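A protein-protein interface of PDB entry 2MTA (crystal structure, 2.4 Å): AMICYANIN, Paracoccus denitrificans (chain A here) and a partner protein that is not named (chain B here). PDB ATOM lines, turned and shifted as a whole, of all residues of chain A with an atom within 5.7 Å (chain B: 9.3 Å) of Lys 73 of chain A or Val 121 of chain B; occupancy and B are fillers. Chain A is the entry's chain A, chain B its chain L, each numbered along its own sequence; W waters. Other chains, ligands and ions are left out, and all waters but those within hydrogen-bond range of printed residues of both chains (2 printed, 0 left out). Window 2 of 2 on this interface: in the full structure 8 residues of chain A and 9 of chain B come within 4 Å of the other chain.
The backbone carbonyl oxygen (O) of Leu 65 of chain B sits at hydrogen-bond distance from the backbone NH (N) of Val 121 of chain B (2.7 Å).
The backbone NH (N) of Leu 65 of chain B is in hydrogen-bond range of the backbone carbonyl oxygen (O) of Gly 122 of chain B (2.7 Å).
OD1 of Asn 47 of chain A sits close to O of Met 51 of chain A (3.0 Å).
N of Lys 73 of chain A sits close to NE2 of Gln 76 of chain A, 3.1 Å away.
Leu 65 of chain B touches Ala 50 of chain A (CD2 to O, 3.4 Å).
Met 51 of chain A touches Val 52 of chain B (CE to CG2, 3.8 Å).
Met 51 of chain A touches Leu 65 of chain B.
Val 121 of chain B touches Pro 52 of chain A.
CG of Met 71 of chain A touches O of Thr 48 of chain B, 3.5 Å away.
Lys 73 of chain A touches Val 121 of chain B.
Lys 73 of chain A touches just one residue of chain B: Val 121 (3.3 Å).
No residue of chain B comes within 4 Å of Asn 47 of chain A.
No residue of chain B comes within 4 Å of Gln 76 of chain A.
Of the printed residues of chain B, Ala 50 of chain A touches Leu 65 (3.4 Å).
Of the printed residues of chain A, Val 52 of chain B touches Met 51.
Of the printed residues of chain B, Pro 52 of chain A touches Val 121.
Of the printed residues of chain A, Leu 65 of chain B touches Ala 50 (3.4 Å) and Met 51 (3.8 Å).
Printed residues of chain B within 4 Å of Met 71 of chain A: Thr 48 (3.5 Å).
Arg 21 of chain B touches none of the printed residues of chain A.
Ile 66 of chain B touches none of the printed residues of chain A.
The nearest residue of chain A that does not touch Val 121 of chain B is Ala 50 of chain A (4.1 Å).
The nearest printed residue of chain A that does not touch Thr 48 of chain B is Pro 52 of chain A (6.3 Å).
Hydrophobic or aromatic side chains of chain A that line the printed part of chain B: Ala 50, Met 51, Pro 52 and Met 71.
Hydrophobic or aromatic side chains of chain B within 4 Å of the printed part of chain A: Val 52, Leu 65 and Val 121.
Among the printed residues, 6 pairs touch across the chains.
Among the printed residues, no Asp or Glu carboxylate lies within 4 Å of a Lys or Arg side-chain nitrogen of the other chain.
Water W1 lies within hydrogen-bond range of O of Ala 50 of chain A (2.6 Å), O of Val 121 of chain B (2.8 Å) and N of Lys 74 of chain A (2.8 Å).
Water W2 lies within hydrogen-bond range of the backbone carbonyl oxygen of Ser 50 of chain B and the side-chain sulfur of Met 51 of chain A.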
ATOM      1  N   ASN A  47     -23.127   2.454  -2.246  1.00  0.00           N
ATOM      2  CA  ASN A  47     -23.108   2.481  -0.800  1.00  0.00           C
ATOM      3  C   ASN A  47     -21.679   2.700  -0.481  1.00  0.00           C
ATOM      4  O   ASN A  47     -20.851   1.895  -0.862  1.00  0.00           O
ATOM      5  CB  ASN A  47     -23.653   1.150  -0.258  1.00  0.00           C
ATOM      6  CG  ASN A  47     -23.443   0.937   1.196  1.00  0.00           C
ATOM      7  OD1 ASN A  47     -23.435  -0.193   1.670  1.00  0.00           O
ATOM      8  ND2 ASN A  47     -23.292   1.939   2.039  1.00  0.00           N
ATOM      9  N   GLU A  49     -20.506   2.989   2.652  1.00  0.00           N
ATOM     10  CA  GLU A  49     -19.981   2.561   3.921  1.00  0.00           C
ATOM     11  C   GLU A  49     -20.139   1.065   3.989  1.00  0.00           C
ATOM     12  O   GLU A  49     -20.810   0.492   3.143  1.00  0.00           O
ATOM     13  CB  GLU A  49     -20.711   3.273   5.055  1.00  0.00           C
ATOM     14  CG  GLU A  49     -22.219   3.261   4.932  1.00  0.00           C
ATOM     15  CD  GLU A  49     -22.946   3.900   6.118  1.00  0.00           C
ATOM     16  OE1 GLU A  49     -22.350   4.251   7.148  1.00  0.00           O
ATOM     17  OE2 GLU A  49     -24.157   4.075   5.986  1.00  0.00           O
ATOM     18  N   ALA A  50     -19.439   0.558   5.012  1.00  0.00           N
ATOM     19  CA  ALA A  50     -19.319  -0.841   5.371  1.00  0.00           C
ATOM     20  C   ALA A  50     -20.632  -1.536   5.698  1.00  0.00           C
ATOM     21  O   ALA A  50     -20.841  -2.702   5.387  1.00  0.00           O
ATOM     22  CB  ALA A  50     -18.378  -0.958   6.583  1.00  0.00           C
ATOM     23  N   MET A  51     -21.505  -0.807   6.390  1.00  0.00           N
ATOM     24  CA  MET A  51     -22.842  -1.197   6.826  1.00  0.00           C
ATOM     25  C   MET A  51     -23.601  -1.499   5.556  1.00  0.00           C
ATOM     26  O   MET A  51     -23.621  -0.642   4.665  1.00  0.00           O
ATOM     27  CB  MET A  51     -23.417  -0.017   7.552  1.00  0.00           C
ATOM     28  CG  MET A  51     -24.870   0.061   7.978  1.00  0.00           C
ATOM     29  SD  MET A  51     -25.249  -1.073   9.321  1.00  0.00           S
ATOM     30  CE  MET A  51     -24.350  -0.397  10.694  1.00  0.00           C
ATOM     31  N   PRO A  52     -24.120  -2.706   5.373  1.00  0.00           N
ATOM     32  CA  PRO A  52     -24.833  -3.004   4.144  1.00  0.00           C
ATOM     33  C   PRO A  52     -26.169  -2.274   4.120  1.00  0.00           C
ATOM     34  O   PRO A  52     -26.877  -2.156   5.124  1.00  0.00           O
ATOM     35  CB  PRO A  52     -24.897  -4.544   4.145  1.00  0.00           C
ATOM     36  CG  PRO A  52     -23.676  -4.903   4.960  1.00  0.00           C
ATOM     37  CD  PRO A  52     -23.768  -3.908   6.120  1.00  0.00           C
ATOM     38  N   HIS A  53     -26.583  -1.781   2.966  1.00  0.00           N
ATOM     39  CA  HIS A  53     -27.842  -1.047   2.806  1.00  0.00           C
ATOM     40  C   HIS A  53     -28.452  -1.420   1.475  1.00  0.00           C
ATOM     41  O   HIS A  53     -27.694  -1.753   0.580  1.00  0.00           O
ATOM     42  CB  HIS A  53     -27.672   0.521   2.748  1.00  0.00           C
ATOM     43  CG  HIS A  53     -27.102   1.243   3.973  1.00  0.00           C
ATOM     44  ND1 HIS A  53     -27.752   1.232   5.112  1.00  0.00           N
ATOM     45  CD2 HIS A  53     -25.856   1.809   4.054  1.00  0.00           C
ATOM     46  CE1 HIS A  53     -26.926   1.782   5.968  1.00  0.00           C
ATOM     47  NE2 HIS A  53     -25.826   2.104   5.336  1.00  0.00           N
ATOM     48  N   MET A  71     -28.778  -6.370  -1.289  1.00  0.00           N
ATOM     49  CA  MET A  71     -28.018  -5.560  -0.371  1.00  0.00           C
ATOM     50  C   MET A  71     -26.722  -5.194  -1.028  1.00  0.00           C
ATOM     51  O   MET A  71     -26.170  -6.007  -1.770  1.00  0.00           O
ATOM     52  CB  MET A  71     -27.733  -6.285   0.906  1.00  0.00           C
ATOM     53  CG  MET A  71     -29.049  -6.428   1.712  1.00  0.00           C
ATOM     54  SD  MET A  71     -29.908  -4.993   2.495  1.00  0.00           S
ATOM     55  CE  MET A  71     -28.806  -4.667   3.815  1.00  0.00           C
ATOM     56  N   MET A  72     -26.296  -3.948  -0.895  1.00  0.00           N
ATOM     57  CA  MET A  72     -25.046  -3.459  -1.417  1.00  0.00           C
ATOM     58  C   MET A  72     -24.179  -3.465  -0.217  1.00  0.00           C
ATOM     59  O   MET A  72     -24.582  -3.396   0.947  1.00  0.00           O
ATOM     60  CB  MET A  72     -25.155  -2.063  -1.910  1.00  0.00           C
ATOM     61  CG  MET A  72     -26.295  -1.984  -2.869  1.00  0.00           C
ATOM     62  SD  MET A  72     -26.511  -0.294  -3.480  1.00  0.00           S
ATOM     63  CE  MET A  72     -28.107  -0.019  -2.836  1.00  0.00           C
ATOM     64  N   LYS A  73     -22.929  -3.611  -0.481  1.00  0.00           N
ATOM     65  CA  LYS A  73     -21.942  -3.604   0.586  1.00  0.00           C
ATOM     66  C   LYS A  73     -21.020  -2.461   0.121  1.00  0.00           C
ATOM     67  O   LYS A  73     -21.258  -1.825  -0.951  1.00  0.00           O
ATOM     68  CB  LYS A  73     -21.409  -4.982   0.498  1.00  0.00           C
ATOM     69  CG  LYS A  73     -20.198  -5.446   1.215  1.00  0.00           C
ATOM     70  CD  LYS A  73     -19.597  -6.614   0.417  1.00  0.00           C
ATOM     71  CE  LYS A  73     -20.503  -7.836   0.372  1.00  0.00           C
ATOM     72  NZ  LYS A  73     -19.961  -8.830  -0.547  1.00  0.00           N
ATOM     73  N   LYS A  74     -19.964  -2.176   0.868  1.00  0.00           N
ATOM     74  CA  LYS A  74     -19.129  -1.069   0.514  1.00  0.00           C
ATOM     75  C   LYS A  74     -18.566  -1.105  -0.887  1.00  0.00           C
ATOM     76  O   LYS A  74     -17.949  -2.035  -1.400  1.00  0.00           O
ATOM     77  CB  LYS A  74     -18.028  -0.987   1.488  1.00  0.00           C
ATOM     78  CG  LYS A  74     -17.406   0.430   1.459  1.00  0.00           C
ATOM     79  CD  LYS A  74     -16.394   0.582   2.573  1.00  0.00           C
ATOM     80  CE  LYS A  74     -15.692   1.941   2.542  1.00  0.00           C
ATOM     81  NZ  LYS A  74     -14.908   2.176   3.757  1.00  0.00           N
ATOM     82  N   GLU A  75     -18.898   0.021  -1.471  1.00  0.00           N
ATOM     83  CA  GLU A  75     -18.525   0.462  -2.784  1.00  0.00           C
ATOM     84  C   GLU A  75     -19.217  -0.359  -3.815  1.00  0.00           C
ATOM     85  O   GLU A  75     -18.715  -0.582  -4.923  1.00  0.00           O
ATOM     86  CB  GLU A  75     -17.025   0.385  -2.987  1.00  0.00           C
ATOM     87  CG  GLU A  75     -16.145   1.307  -2.143  1.00  0.00           C
ATOM     88  CD  GLU A  75     -16.018   2.711  -2.694  1.00  0.00           C
ATOM     89  OE1 GLU A  75     -15.454   2.868  -3.781  1.00  0.00           O
ATOM     90  OE2 GLU A  75     -16.475   3.644  -2.036  1.00  0.00           O
ATOM     91  N   GLN A  76     -20.403  -0.814  -3.510  1.00  0.00           N
ATOM     92  CA  GLN A  76     -21.151  -1.430  -4.581  1.00  0.00           C
ATOM     93  C   GLN A  76     -22.304  -0.526  -4.965  1.00  0.00           C
ATOM     94  O   GLN A  76     -22.791   0.229  -4.106  1.00  0.00           O
ATOM     95  CB  GLN A  76     -21.669  -2.746  -4.128  1.00  0.00           C
ATOM     96  CG  GLN A  76     -20.607  -3.782  -3.857  1.00  0.00           C
ATOM     97  CD  GLN A  76     -21.174  -5.037  -3.200  1.00  0.00           C
ATOM     98  OE1 GLN A  76     -20.437  -5.871  -2.684  1.00  0.00           O
ATOM     99  NE2 GLN A  76     -22.461  -5.300  -3.068  1.00  0.00           N
ATOM    100  N   ALA A  77     -22.775  -0.731  -6.194  1.00  0.00           N
ATOM    101  CA  ALA A  77     -23.839   0.041  -6.841  1.00  0.00           C
ATOM    102  C   ALA A  77     -25.057  -0.759  -7.291  1.00  0.00           C
ATOM    103  O   ALA A  77     -25.037  -1.994  -7.252  1.00  0.00           O
ATOM    104  CB  ALA A  77     -23.360   0.744  -8.101  1.00  0.00           C
ATOM    105  N   TRP B  20     -14.978 -16.336  17.314  1.00  0.00           N
ATOM    106  CA  TRP B  20     -14.893 -14.941  16.975  1.00  0.00           C
ATOM    107  C   TRP B  20     -15.897 -14.379  15.976  1.00  0.00           C
ATOM    108  O   TRP B  20     -16.351 -13.248  16.203  1.00  0.00           O
ATOM    109  CB  TRP B  20     -13.449 -14.648  16.498  1.00  0.00           C
ATOM    110  CG  TRP B  20     -13.101 -14.663  15.012  1.00  0.00           C
ATOM    111  CD1 TRP B  20     -12.474 -15.749  14.527  1.00  0.00           C
ATOM    112  CD2 TRP B  20     -13.316 -13.700  14.030  1.00  0.00           C
ATOM    113  NE1 TRP B  20     -12.290 -15.496  13.252  1.00  0.00           N
ATOM    114  CE2 TRP B  20     -12.766 -14.320  12.905  1.00  0.00           C
ATOM    115  CE3 TRP B  20     -13.883 -12.431  13.897  1.00  0.00           C
ATOM    116  CZ2 TRP B  20     -12.764 -13.729  11.655  1.00  0.00           C
ATOM    117  CZ3 TRP B  20     -13.887 -11.832  12.665  1.00  0.00           C
ATOM    118  CH2 TRP B  20     -13.339 -12.469  11.560  1.00  0.00           C
ATOM    119  N   ARG B  21     -16.333 -15.000  14.884  1.00  0.00           N
ATOM    120  CA  ARG B  21     -17.281 -14.247  14.069  1.00  0.00           C
ATOM    121  C   ARG B  21     -18.624 -14.210  14.767  1.00  0.00           C
ATOM    122  O   ARG B  21     -19.497 -13.583  14.187  1.00  0.00           O
ATOM    123  CB  ARG B  21     -17.573 -14.818  12.674  1.00  0.00           C
ATOM    124  CG  ARG B  21     -16.380 -15.165  11.889  1.00  0.00           C
ATOM    125  CD  ARG B  21     -16.737 -15.162  10.409  1.00  0.00           C
ATOM    126  NE  ARG B  21     -15.526 -15.563   9.706  1.00  0.00           N
ATOM    127  CZ  ARG B  21     -15.460 -15.680   8.386  1.00  0.00           C
ATOM    128  NH1 ARG B  21     -16.529 -15.451   7.631  1.00  0.00           N
ATOM    129  NH2 ARG B  21     -14.275 -15.934   7.820  1.00  0.00           N
ATOM    130  N   THR B  38     -21.258 -19.664   6.211  1.00  0.00           N
ATOM    131  CA  THR B  38     -21.816 -18.572   5.436  1.00  0.00           C
ATOM    132  C   THR B  38     -22.977 -18.948   4.620  1.00  0.00           C
ATOM    133  O   THR B  38     -23.394 -18.157   3.786  1.00  0.00           O
ATOM    134  CB  THR B  38     -20.685 -17.946   4.522  1.00  0.00           C
ATOM    135  OG1 THR B  38     -20.246 -18.844   3.484  1.00  0.00           O
ATOM    136  CG2 THR B  38     -19.499 -17.571   5.421  1.00  0.00           C
ATOM    137  N   THR B  48     -31.982 -11.240   3.174  1.00  0.00           N
ATOM    138  CA  THR B  48     -31.047 -10.245   2.691  1.00  0.00           C
ATOM    139  C   THR B  48     -30.622  -9.277   3.823  1.00  0.00           C
ATOM    140  O   THR B  48     -29.445  -8.959   4.060  1.00  0.00           O
ATOM    141  CB  THR B  48     -31.783  -9.653   1.502  1.00  0.00           C
ATOM    142  OG1 THR B  48     -33.150  -9.314   1.796  1.00  0.00           O
ATOM    143  CG2 THR B  48     -31.728 -10.734   0.399  1.00  0.00           C
ATOM    144  N   SER B  50     -30.033  -7.710   7.771  1.00  0.00           N
ATOM    145  CA  SER B  50     -29.317  -8.174   8.935  1.00  0.00           C
ATOM    146  C   SER B  50     -29.011  -7.144  10.002  1.00  0.00           C
ATOM    147  O   SER B  50     -29.080  -5.957   9.699  1.00  0.00           O
ATOM    148  CB  SER B  50     -27.986  -8.794   8.494  1.00  0.00           C
ATOM    149  OG  SER B  50     -27.422  -8.106   7.343  1.00  0.00           O
ATOM    150  N   TRQ B  51     -28.769  -7.605  11.240  1.00  0.00           N
ATOM    151  CA  TRQ B  51     -28.136  -6.760  12.218  1.00  0.00           C
ATOM    152  C   TRQ B  51     -26.656  -6.944  11.977  1.00  0.00           C
ATOM    153  O   TRQ B  51     -26.323  -7.888  11.259  1.00  0.00           O
ATOM    154  CB  TRQ B  51     -28.450  -7.162  13.655  1.00  0.00           C
ATOM    155  CG  TRQ B  51     -28.248  -8.581  14.201  1.00  0.00           C
ATOM    156  CD1 TRQ B  51     -27.116  -8.840  14.958  1.00  0.00           C
ATOM    157  NE1 TRQ B  51     -27.185 -10.096  15.265  1.00  0.00           N
ATOM    158  CE2 TRQ B  51     -28.297 -10.623  14.723  1.00  0.00           C
ATOM    159  CZ2 TRQ B  51     -28.612 -11.979  14.865  1.00  0.00           C
ATOM    160  CH2 TRQ B  51     -29.793 -12.359  14.248  1.00  0.00           C
ATOM    161  CZ3 TRQ B  51     -30.602 -11.456  13.612  1.00  0.00           C
ATOM    162  CE3 TRQ B  51     -30.277 -10.151  13.452  1.00  0.00           C
ATOM    163  CD2 TRQ B  51     -29.085  -9.665  14.026  1.00  0.00           C
ATOM    164  O6  TRQ B  51     -30.140 -13.546  14.224  1.00  0.00           O
ATOM    165  O7  TRQ B  51     -27.798 -12.788  15.366  1.00  0.00           O
ATOM    166  N   VAL B  52     -25.728  -6.118  12.447  1.00  0.00           N
ATOM    167  CA  VAL B  52     -24.322  -6.351  12.229  1.00  0.00           C
ATOM    168  C   VAL B  52     -23.621  -6.263  13.557  1.00  0.00           C
ATOM    169  O   VAL B  52     -24.261  -6.011  14.569  1.00  0.00           O
ATOM    170  CB  VAL B  52     -23.634  -5.339  11.231  1.00  0.00           C
ATOM    171  CG1 VAL B  52     -24.327  -5.359   9.867  1.00  0.00           C
ATOM    172  CG2 VAL B  52     -23.657  -3.965  11.793  1.00  0.00           C
ATOM    173  N   ALA B  53     -22.322  -6.530  13.602  1.00  0.00           N
ATOM    174  CA  ALA B  53     -21.436  -6.436  14.755  1.00  0.00           C
ATOM    175  C   ALA B  53     -20.025  -6.289  14.198  1.00  0.00           C
ATOM    176  O   ALA B  53     -19.830  -6.531  13.003  1.00  0.00           O
ATOM    177  CB  ALA B  53     -21.409  -7.696  15.609  1.00  0.00           C
ATOM    178  N   SER B  54     -19.071  -5.842  15.011  1.00  0.00           N
ATOM    179  CA  SER B  54     -17.674  -5.725  14.640  1.00  0.00           C
ATOM    180  C   SER B  54     -17.017  -6.645  15.605  1.00  0.00           C
ATOM    181  O   SER B  54     -17.140  -6.482  16.830  1.00  0.00           O
ATOM    182  CB  SER B  54     -17.098  -4.335  14.874  1.00  0.00           C
ATOM    183  OG  SER B  54     -17.513  -3.559  13.751  1.00  0.00           O
ATOM    184  N   SER B  63     -10.623  -6.079  13.578  1.00  0.00           N
ATOM    185  CA  SER B  63     -12.040  -6.160  13.757  1.00  0.00           C
ATOM    186  C   SER B  63     -12.652  -6.227  12.381  1.00  0.00           C
ATOM    187  O   SER B  63     -12.161  -5.553  11.455  1.00  0.00           O
ATOM    188  CB  SER B  63     -12.539  -4.941  14.484  1.00  0.00           C
ATOM    189  OG  SER B  63     -12.167  -4.884  15.863  1.00  0.00           O
ATOM    190  N   TYR B  64     -13.695  -7.065  12.238  1.00  0.00           N
ATOM    191  CA  TYR B  64     -14.419  -7.209  10.972  1.00  0.00           C
ATOM    192  C   TYR B  64     -15.866  -6.962  11.200  1.00  0.00           C
ATOM    193  O   TYR B  64     -16.340  -7.161  12.314  1.00  0.00           O
ATOM    194  CB  TYR B  64     -14.358  -8.586  10.401  1.00  0.00           C
ATOM    195  CG  TYR B  64     -12.972  -8.856   9.876  1.00  0.00           C
ATOM    196  CD1 TYR B  64     -11.972  -9.281  10.757  1.00  0.00           C
ATOM    197  CD2 TYR B  64     -12.734  -8.638   8.532  1.00  0.00           C
ATOM    198  CE1 TYR B  64     -10.705  -9.488  10.282  1.00  0.00           C
ATOM    199  CE2 TYR B  64     -11.460  -8.859   8.045  1.00  0.00           C
ATOM    200  CZ  TYR B  64     -10.473  -9.275   8.922  1.00  0.00           C
ATOM    201  OH  TYR B  64      -9.190  -9.488   8.437  1.00  0.00           O
ATOM    202  N   LEU B  65     -16.577  -6.583  10.156  1.00  0.00           N
ATOM    203  CA  LEU B  65     -18.004  -6.392  10.248  1.00  0.00           C
ATOM    204  C   LEU B  65     -18.669  -7.690   9.804  1.00  0.00           C
ATOM    205  O   LEU B  65     -18.533  -8.130   8.643  1.00  0.00           O
ATOM    206  CB  LEU B  65     -18.466  -5.254   9.334  1.00  0.00           C
ATOM    207  CG  LEU B  65     -19.719  -4.471   9.683  1.00  0.00           C
ATOM    208  CD1 LEU B  65     -19.474  -3.677  10.960  1.00  0.00           C
ATOM    209  CD2 LEU B  65     -20.065  -3.510   8.588  1.00  0.00           C
ATOM    210  N   ILE B  66     -19.416  -8.272  10.734  1.00  0.00           N
ATOM    211  CA  ILE B  66     -20.159  -9.510  10.526  1.00  0.00           C
ATOM    212  C   ILE B  66     -21.596  -9.142  10.149  1.00  0.00           C
ATOM    213  O   ILE B  66     -22.158  -8.345  10.880  1.00  0.00           O
ATOM    214  CB  ILE B  66     -20.144 -10.307  11.830  1.00  0.00           C
ATOM    215  CG1 ILE B  66     -18.755 -10.400  12.459  1.00  0.00           C
ATOM    216  CG2 ILE B  66     -20.730 -11.678  11.507  1.00  0.00           C
ATOM    217  CD1 ILE B  66     -17.656 -10.990  11.498  1.00  0.00           C
ATOM    218  N   ALA B  67     -22.296  -9.627   9.108  1.00  0.00           N
ATOM    219  CA  ALA B  67     -23.697  -9.311   8.831  1.00  0.00           C
ATOM    220  C   ALA B  67     -24.518 -10.559   9.203  1.00  0.00           C
ATOM    221  O   ALA B  67     -24.588 -11.532   8.432  1.00  0.00           O
ATOM    222  CB  ALA B  67     -23.930  -9.037   7.342  1.00  0.00           C
ATOM    223  N   TYR B  68     -25.186 -10.582  10.370  1.00  0.00           N
ATOM    224  CA  TYR B  68     -25.931 -11.736  10.851  1.00  0.00           C
ATOM    225  C   TYR B  68     -27.286 -11.856  10.200  1.00  0.00           C
ATOM    226  O   TYR B  68     -28.333 -11.423  10.691  1.00  0.00           O
ATOM    227  CB  TYR B  68     -26.191 -11.714  12.366  1.00  0.00           C
ATOM    228  CG  TYR B  68     -24.898 -11.715  13.145  1.00  0.00           C
ATOM    229  CD1 TYR B  68     -24.310 -12.897  13.513  1.00  0.00           C
ATOM    230  CD2 TYR B  68     -24.285 -10.519  13.487  1.00  0.00           C
ATOM    231  CE1 TYR B  68     -23.116 -12.868  14.231  1.00  0.00           C
ATOM    232  CE2 TYR B  68     -23.100 -10.501  14.183  1.00  0.00           C
ATOM    233  CZ  TYR B  68     -22.521 -11.670  14.558  1.00  0.00           C
ATOM    234  OH  TYR B  68     -21.363 -11.623  15.300  1.00  0.00           O
ATOM    235  N   ARG B  69     -27.189 -12.467   9.046  1.00  0.00           N
ATOM    236  CA  ARG B  69     -28.344 -12.832   8.268  1.00  0.00           C
ATOM    237  C   ARG B  69     -28.998 -14.121   8.744  1.00  0.00           C
ATOM    238  O   ARG B  69     -28.299 -15.098   9.026  1.00  0.00           O
ATOM    239  CB  ARG B  69     -27.880 -12.963   6.852  1.00  0.00           C
ATOM    240  CG  ARG B  69     -27.231 -11.711   6.247  1.00  0.00           C
ATOM    241  CD  ARG B  69     -27.764 -12.066   4.926  1.00  0.00           C
ATOM    242  NE  ARG B  69     -26.632 -12.239   4.062  1.00  0.00           N
ATOM    243  CZ  ARG B  69     -26.791 -12.396   2.758  1.00  0.00           C
ATOM    244  NH1 ARG B  69     -27.988 -12.446   2.144  1.00  0.00           N
ATOM    245  NH2 ARG B  69     -25.661 -12.366   2.061  1.00  0.00           N
ATOM    246  N   ILE B 117     -26.390 -17.111  10.026  1.00  0.00           N
ATOM    247  CA  ILE B 117     -25.084 -17.395   9.435  1.00  0.00           C
ATOM    248  C   ILE B 117     -24.146 -16.268   9.863  1.00  0.00           C
ATOM    249  O   ILE B 117     -24.644 -15.369  10.528  1.00  0.00           O
ATOM    250  CB  ILE B 117     -25.178 -17.465   7.928  1.00  0.00           C
ATOM    251  CG1 ILE B 117     -25.712 -16.241   7.317  1.00  0.00           C
ATOM    252  CG2 ILE B 117     -26.178 -18.562   7.611  1.00  0.00           C
ATOM    253  CD1 ILE B 117     -25.550 -16.170   5.793  1.00  0.00           C
ATOM    254  N   SER B 118     -22.824 -16.236   9.589  1.00  0.00           N
ATOM    255  CA  SER B 118     -21.922 -15.181  10.059  1.00  0.00           C
ATOM    256  C   SER B 118     -21.020 -14.726   8.920  1.00  0.00           C
ATOM    257  O   SER B 118     -19.798 -14.784   9.075  1.00  0.00           O
ATOM    258  CB  SER B 118     -21.032 -15.664  11.223  1.00  0.00           C
ATOM    259  OG  SER B 118     -21.711 -16.298  12.326  1.00  0.00           O
ATOM    260  N   PRO B 119     -21.485 -14.291   7.755  1.00  0.00           N
ATOM    261  CA  PRO B 119     -20.613 -13.826   6.730  1.00  0.00           C
ATOM    262  C   PRO B 119     -19.861 -12.554   7.157  1.00  0.00           C
ATOM    263  O   PRO B 119     -20.342 -11.794   8.008  1.00  0.00           O
ATOM    264  CB  PRO B 119     -21.555 -13.693   5.564  1.00  0.00           C
ATOM    265  CG  PRO B 119     -22.850 -13.241   6.197  1.00  0.00           C
ATOM    266  CD  PRO B 119     -22.864 -14.145   7.399  1.00  0.00           C
ATOM    267  N   ILE B 120     -18.653 -12.301   6.665  1.00  0.00           N
ATOM    268  CA  ILE B 120     -17.921 -11.082   6.888  1.00  0.00           C
ATOM    269  C   ILE B 120     -18.392 -10.153   5.759  1.00  0.00           C
ATOM    270  O   ILE B 120     -18.376 -10.624   4.601  1.00  0.00           O
ATOM    271  CB  ILE B 120     -16.417 -11.337   6.772  1.00  0.00           C
ATOM    272  CG1 ILE B 120     -15.918 -12.010   8.041  1.00  0.00           C
ATOM    273  CG2 ILE B 120     -15.666 -10.021   6.608  1.00  0.00           C
ATOM    274  CD1 ILE B 120     -14.371 -12.287   7.989  1.00  0.00           C
ATOM    275  N   VAL B 121     -18.888  -8.911   6.066  1.00  0.00           N
ATOM    276  CA  VAL B 121     -19.227  -7.928   5.004  1.00  0.00           C
ATOM    277  C   VAL B 121     -18.205  -6.802   4.809  1.00  0.00           C
ATOM    278  O   VAL B 121     -18.346  -6.072   3.833  1.00  0.00           O
ATOM    279  CB  VAL B 121     -20.599  -7.181   5.146  1.00  0.00           C
ATOM    280  CG1 VAL B 121     -21.650  -8.178   4.714  1.00  0.00           C
ATOM    281  CG2 VAL B 121     -20.889  -6.648   6.533  1.00  0.00           C
ATOM    282  N   GLY B 122     -17.178  -6.608   5.637  1.00  0.00           N
ATOM    283  CA  GLY B 122     -16.122  -5.658   5.358  1.00  0.00           C
ATOM    284  C   GLY B 122     -15.332  -5.507   6.636  1.00  0.00           C
ATOM    285  O   GLY B 122     -15.715  -6.130   7.651  1.00  0.00           O
ATOM    286  N   LYS B 123     -14.228  -4.733   6.614  1.00  0.00           N
ATOM    287  CA  LYS B 123     -13.403  -4.509   7.816  1.00  0.00           C
ATOM    288  C   LYS B 123     -13.926  -3.283   8.539  1.00  0.00           C
ATOM    289  O   LYS B 123     -14.489  -2.392   7.903  1.00  0.00           O
ATOM    290  CB  LYS B 123     -11.924  -4.255   7.492  1.00  0.00           C
ATOM    291  CG  LYS B 123     -10.989  -4.282   8.753  1.00  0.00           C
ATOM    292  CD  LYS B 123      -9.501  -4.000   8.477  1.00  0.00           C
ATOM    293  CE  LYS B 123      -8.945  -4.986   7.410  1.00  0.00           C
ATOM    294  NZ  LYS B 123      -7.517  -4.859   7.122  1.00  0.00           N
ATOM    295  N   ALA B 124     -13.814  -3.224   9.849  1.00  0.00           N
ATOM    296  CA  ALA B 124     -14.254  -2.061  10.594  1.00  0.00           C
ATOM    297  C   ALA B 124     -13.449  -2.120  11.882  1.00  0.00           C
ATOM    298  O   ALA B 124     -13.931  -2.781  12.819  1.00  0.00           O
ATOM    299  CB  ALA B 124     -15.740  -2.180  10.905  1.00  0.00           C
HETATM  300  O   HOH W   1     -19.486  -3.560   3.294  1.00  0.00           O
HETATM  301  O   HOH W   2     -27.888  -3.459  10.095  1.00  0.00           O
